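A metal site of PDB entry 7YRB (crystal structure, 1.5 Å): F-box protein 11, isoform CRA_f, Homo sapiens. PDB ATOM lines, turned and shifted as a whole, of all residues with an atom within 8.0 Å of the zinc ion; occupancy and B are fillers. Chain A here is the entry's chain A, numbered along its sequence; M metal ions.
Four residues have an atom within 4 Å of the zinc ion: Cys 32, Cys 35, His 52 and His 55. The nearest printed residue that does not touch the zinc ion is Thr 34 (4.3 Å).
The side-chain sulfur (SG) of Cys 32 sits close to the backbone NH (N) of Thr 34 (3.5 Å). N of Cys 32 sits at hydrogen-bond distance from OD1 of Asn 41 (2.9 Å). A ring nitrogen (NE2) of His 52 sits close to the side-chain sulfur (SG) of Cys 69. The backbone carbonyl oxygen of Cys 32 lies close to the side-chain amide oxygen of Asn 36. O of Cys 47 is in hydrogen-bond range of N of His 52, at 3.1 Å.
The zinc ion is bound by a ring nitrogen (ND1) of His 55, a ring nitrogen (ND1) of His 52, the side-chain sulfur of Cys 32 and the side-chain sulfur of Cys 35. The zinc ion has four donor atoms within binding distance.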
ATOM      1  N   ARG A  31      11.033  24.979  12.459  1.00  0.00           N
ATOM      2  CA  ARG A  31      10.893  23.703  11.787  1.00  0.00           C
ATOM      3  C   ARG A  31      11.612  22.665  12.625  1.00  0.00           C
ATOM      4  O   ARG A  31      12.690  22.932  13.140  1.00  0.00           O
ATOM      5  CB  ARG A  31      11.511  23.781  10.416  1.00  0.00           C
ATOM      6  CG  ARG A  31      11.371  22.573   9.546  1.00  0.00           C
ATOM      7  CD  ARG A  31      11.347  22.994   8.063  1.00  0.00           C
ATOM      8  NE  ARG A  31      10.092  23.679   7.791  1.00  0.00           N
ATOM      9  CZ  ARG A  31       9.908  24.672   6.928  1.00  0.00           C
ATOM     10  NH1 ARG A  31      10.859  25.073   6.102  1.00  0.00           N
ATOM     11  NH2 ARG A  31       8.731  25.282   6.914  1.00  0.00           N
ATOM     12  N   CYS A  32      11.019  21.478  12.757  1.00  0.00           N
ATOM     13  CA  CYS A  32      11.683  20.373  13.436  1.00  0.00           C
ATOM     14  C   CYS A  32      11.954  19.293  12.399  1.00  0.00           C
ATOM     15  O   CYS A  32      11.021  18.748  11.793  1.00  0.00           O
ATOM     16  CB  CYS A  32      10.869  19.833  14.603  1.00  0.00           C
ATOM     17  SG  CYS A  32      11.803  18.468  15.382  1.00  0.00           S
ATOM     18  N   HIS A  33      13.242  19.006  12.195  1.00  0.00           N
ATOM     19  CA  HIS A  33      13.672  17.958  11.271  1.00  0.00           C
ATOM     20  C   HIS A  33      13.608  16.579  11.881  1.00  0.00           C
ATOM     21  O   HIS A  33      13.603  15.577  11.148  1.00  0.00           O
ATOM     22  CB  HIS A  33      15.094  18.245  10.823  1.00  0.00           C
ATOM     23  CG  HIS A  33      15.246  19.569  10.160  1.00  0.00           C
ATOM     24  ND1 HIS A  33      14.572  19.881   8.997  1.00  0.00           N
ATOM     25  CD2 HIS A  33      15.937  20.680  10.511  1.00  0.00           C
ATOM     26  CE1 HIS A  33      14.875  21.119   8.641  1.00  0.00           C
ATOM     27  NE2 HIS A  33      15.699  21.626   9.545  1.00  0.00           N
ATOM     28  N   THR A  34      13.615  16.493  13.203  1.00  0.00           N
ATOM     29  CA  THR A  34      13.507  15.208  13.869  1.00  0.00           C
ATOM     30  C   THR A  34      12.123  14.614  13.710  1.00  0.00           C
ATOM     31  O   THR A  34      11.971  13.397  13.619  1.00  0.00           O
ATOM     32  CB  THR A  34      13.822  15.386  15.343  1.00  0.00           C
ATOM     33  OG1 THR A  34      15.136  15.947  15.490  1.00  0.00           O
ATOM     34  CG2 THR A  34      13.771  14.055  16.038  1.00  0.00           C
ATOM     35  N   CYS A  35      11.086  15.460  13.715  1.00  0.00           N
ATOM     36  CA  CYS A  35       9.697  15.048  13.714  1.00  0.00           C
ATOM     37  C   CYS A  35       9.074  15.146  12.341  1.00  0.00           C
ATOM     38  O   CYS A  35       7.848  15.253  12.230  1.00  0.00           O
ATOM     39  CB  CYS A  35       8.888  15.905  14.708  1.00  0.00           C
ATOM     40  SG  CYS A  35       9.234  15.692  16.431  1.00  0.00           S
ATOM     41  N   ASN A  36       9.901  15.107  11.288  1.00  0.00           N
ATOM     42  CA  ASN A  36       9.465  15.419   9.916  1.00  0.00           C
ATOM     43  C   ASN A  36       8.694  14.240   9.324  1.00  0.00           C
ATOM     44  O   ASN A  36       9.212  13.407   8.571  1.00  0.00           O
ATOM     45  CB  ASN A  36      10.640  15.763   9.015  1.00  0.00           C
ATOM     46  CG  ASN A  36      10.821  17.264   8.836  1.00  0.00           C
ATOM     47  OD1 ASN A  36       9.879  18.034   9.019  1.00  0.00           O
ATOM     48  ND2 ASN A  36      12.008  17.674   8.396  1.00  0.00           N
ATOM     49  N   ASN A  41       7.162  21.509   8.001  1.00  0.00           N
ATOM     50  CA  ASN A  41       6.315  21.860   9.127  1.00  0.00           C
ATOM     51  C   ASN A  41       6.621  23.277   9.603  1.00  0.00           C
ATOM     52  O   ASN A  41       7.716  23.820   9.376  1.00  0.00           O
ATOM     53  CB  ASN A  41       6.436  20.829  10.289  1.00  0.00           C
ATOM     54  CG  ASN A  41       7.870  20.620  10.826  1.00  0.00           C
ATOM     55  OD1 ASN A  41       8.469  21.494  11.436  1.00  0.00           O
ATOM     56  ND2 ASN A  41       8.358  19.405  10.673  1.00  0.00           N
ATOM     57  N   ILE A  43       6.184  25.388  13.292  1.00  0.00           N
ATOM     58  CA  ILE A  43       5.963  25.157  14.716  1.00  0.00           C
ATOM     59  C   ILE A  43       6.138  26.459  15.486  1.00  0.00           C
ATOM     60  O   ILE A  43       7.098  27.210  15.248  1.00  0.00           O
ATOM     61  CB  ILE A  43       6.916  24.066  15.252  1.00  0.00           C
ATOM     62  CG1 ILE A  43       6.716  22.767  14.444  1.00  0.00           C
ATOM     63  CG2 ILE A  43       6.741  23.824  16.739  1.00  0.00           C
ATOM     64  CD1 ILE A  43       7.696  21.651  14.805  1.00  0.00           C
ATOM     65  N   CYS A  47       6.004  25.646  21.394  1.00  0.00           N
ATOM     66  CA  CYS A  47       6.143  24.234  21.066  1.00  0.00           C
ATOM     67  C   CYS A  47       7.576  23.869  20.759  1.00  0.00           C
ATOM     68  O   CYS A  47       8.060  22.806  21.199  1.00  0.00           O
ATOM     69  CB  CYS A  47       5.246  23.900  19.879  1.00  0.00           C
ATOM     70  SG  CYS A  47       3.520  23.733  20.319  1.00  0.00           S
ATOM     71  N   ILE A  48       8.312  24.720  20.047  1.00  0.00           N
ATOM     72  CA  ILE A  48       9.685  24.324  19.695  1.00  0.00           C
ATOM     73  C   ILE A  48      10.547  24.201  20.937  1.00  0.00           C
ATOM     74  O   ILE A  48      11.469  23.379  20.976  1.00  0.00           O
ATOM     75  CB  ILE A  48      10.284  25.294  18.652  1.00  0.00           C
ATOM     76  CG1 ILE A  48      11.259  24.543  17.727  1.00  0.00           C
ATOM     77  CG2 ILE A  48      10.945  26.492  19.324  1.00  0.00           C
ATOM     78  CD1 ILE A  48      10.581  23.511  16.831  1.00  0.00           C
ATOM     79  N   CYS A  51       7.806  21.042  23.347  1.00  0.00           N
ATOM     80  CA  CYS A  51       7.497  19.810  22.640  1.00  0.00           C
ATOM     81  C   CYS A  51       8.673  19.287  21.844  1.00  0.00           C
ATOM     82  O   CYS A  51       8.721  18.077  21.532  1.00  0.00           O
ATOM     83  CB  CYS A  51       6.315  20.040  21.694  1.00  0.00           C
ATOM     84  SG  CYS A  51       4.921  20.879  22.499  1.00  0.00           S
ATOM     85  N   HIS A  52       9.621  20.144  21.473  1.00  0.00           N
ATOM     86  CA  HIS A  52      10.744  19.728  20.651  1.00  0.00           C
ATOM     87  C   HIS A  52      12.075  20.046  21.310  1.00  0.00           C
ATOM     88  O   HIS A  52      13.088  20.201  20.634  1.00  0.00           O
ATOM     89  CB  HIS A  52      10.638  20.330  19.258  1.00  0.00           C
ATOM     90  CG  HIS A  52       9.338  19.987  18.633  1.00  0.00           C
ATOM     91  ND1 HIS A  52       9.128  18.855  17.889  1.00  0.00           N
ATOM     92  CD2 HIS A  52       8.144  20.640  18.676  1.00  0.00           C
ATOM     93  CE1 HIS A  52       7.868  18.825  17.483  1.00  0.00           C
ATOM     94  NE2 HIS A  52       7.248  19.884  17.982  1.00  0.00           N
ATOM     95  N   GLN A  53      12.071  20.106  22.640  1.00  0.00           N
ATOM     96  CA  GLN A  53      13.313  20.251  23.396  1.00  0.00           C
ATOM     97  C   GLN A  53      14.293  19.153  23.048  1.00  0.00           C
ATOM     98  O   GLN A  53      13.986  17.965  23.181  1.00  0.00           O
ATOM     99  CB  GLN A  53      13.065  20.180  24.891  1.00  0.00           C
ATOM    100  CG  GLN A  53      14.304  20.645  25.648  1.00  0.00           C
ATOM    101  CD  GLN A  53      14.047  20.779  27.112  1.00  0.00           C
ATOM    102  OE1 GLN A  53      14.722  20.182  27.942  1.00  0.00           O
ATOM    103  NE2 GLN A  53      13.044  21.554  27.446  1.00  0.00           N
ATOM    104  N   GLY A  54      15.478  19.564  22.638  1.00  0.00           N
ATOM    105  CA  GLY A  54      16.511  18.611  22.288  1.00  0.00           C
ATOM    106  C   GLY A  54      16.383  18.030  20.894  1.00  0.00           C
ATOM    107  O   GLY A  54      17.210  17.199  20.508  1.00  0.00           O
ATOM    108  N   HIS A  55      15.356  18.401  20.149  1.00  0.00           N
ATOM    109  CA  HIS A  55      15.235  17.950  18.769  1.00  0.00           C
ATOM    110  C   HIS A  55      16.106  18.805  17.869  1.00  0.00           C
ATOM    111  O   HIS A  55      16.651  19.841  18.274  1.00  0.00           O
ATOM    112  CB  HIS A  55      13.798  18.029  18.299  1.00  0.00           C
ATOM    113  CG  HIS A  55      12.863  17.150  19.050  1.00  0.00           C
ATOM    114  ND1 HIS A  55      11.623  16.800  18.565  1.00  0.00           N
ATOM    115  CD2 HIS A  55      13.031  16.440  20.198  1.00  0.00           C
ATOM    116  CE1 HIS A  55      11.031  15.992  19.423  1.00  0.00           C
ATOM    117  NE2 HIS A  55      11.870  15.755  20.423  1.00  0.00           N
ATOM    118  N   ASP A  56      16.221  18.361  16.608  1.00  0.00           N
ATOM    119  CA  ASP A  56      16.940  19.078  15.551  1.00  0.00           C
ATOM    120  C   ASP A  56      16.035  20.143  14.939  1.00  0.00           C
ATOM    121  O   ASP A  56      15.277  19.881  14.006  1.00  0.00           O
ATOM    122  CB  ASP A  56      17.400  18.112  14.464  1.00  0.00           C
ATOM    123  CG  ASP A  56      18.148  18.805  13.343  1.00  0.00           C
ATOM    124  OD1 ASP A  56      18.538  19.982  13.515  1.00  0.00           O
ATOM    125  OD2 ASP A  56      18.349  18.164  12.283  1.00  0.00           O
ATOM    126  N   VAL A  57      16.162  21.373  15.429  1.00  0.00           N
ATOM    127  CA  VAL A  57      15.215  22.429  15.113  1.00  0.00           C
ATOM    128  C   VAL A  57      15.934  23.635  14.519  1.00  0.00           C
ATOM    129  O   VAL A  57      17.125  23.868  14.746  1.00  0.00           O
ATOM    130  CB  VAL A  57      14.408  22.846  16.351  1.00  0.00           C
ATOM    131  CG1 VAL A  57      13.672  21.641  16.929  1.00  0.00           C
ATOM    132  CG2 VAL A  57      15.318  23.474  17.397  1.00  0.00           C
ATOM    133  N   CYS A  69       2.472  21.420  15.261  1.00  0.00           N
ATOM    134  CA  CYS A  69       2.561  20.637  16.495  1.00  0.00           C
ATOM    135  C   CYS A  69       1.223  20.590  17.193  1.00  0.00           C
ATOM    136  O   CYS A  69       0.676  19.518  17.472  1.00  0.00           O
ATOM    137  CB  CYS A  69       3.653  21.213  17.409  1.00  0.00           C
ATOM    138  SG  CYS A  69       4.065  20.223  18.825  1.00  0.00           S
ATOM    139  N   LEU A  74       2.279  16.076  13.607  1.00  0.00           N
ATOM    140  CA  LEU A  74       3.666  15.640  13.689  1.00  0.00           C
ATOM    141  C   LEU A  74       3.788  14.267  14.334  1.00  0.00           C
ATOM    142  O   LEU A  74       2.861  13.748  14.957  1.00  0.00           O
ATOM    143  CB  LEU A  74       4.524  16.636  14.465  1.00  0.00           C
ATOM    144  CG  LEU A  74       4.546  18.091  13.966  1.00  0.00           C
ATOM    145  CD1 LEU A  74       5.477  18.902  14.850  1.00  0.00           C
ATOM    146  CD2 LEU A  74       4.976  18.167  12.523  1.00  0.00           C
ATOM    147  N   SER A  75       4.976  13.689  14.213  1.00  0.00           N
ATOM    148  CA  SER A  75       5.218  12.339  14.710  1.00  0.00           C
ATOM    149  C   SER A  75       4.894  12.211  16.191  1.00  0.00           C
ATOM    150  O   SER A  75       4.557  11.126  16.658  1.00  0.00           O
ATOM    151  CB  SER A  75       6.668  11.943  14.425  1.00  0.00           C
ATOM    152  OG  SER A  75       7.483  12.104  15.567  1.00  0.00           O
ATOM    153  N   ASN A  76       4.961  13.310  16.936  1.00  0.00           N
ATOM    154  CA  ASN A  76       4.867  13.258  18.384  1.00  0.00           C
ATOM    155  C   ASN A  76       3.717  14.136  18.869  1.00  0.00           C
ATOM    156  O   ASN A  76       3.365  15.109  18.213  1.00  0.00           O
ATOM    157  CB  ASN A  76       6.190  13.720  18.991  1.00  0.00           C
ATOM    158  CG  ASN A  76       7.079  12.553  19.394  1.00  0.00           C
ATOM    159  OD1 ASN A  76       6.584  11.535  19.880  1.00  0.00           O
ATOM    160  ND2 ASN A  76       8.389  12.681  19.152  1.00  0.00           N
HETATM  161 ZN    ZN M   1      10.512  17.513  17.005  1.00  0.00          ZN
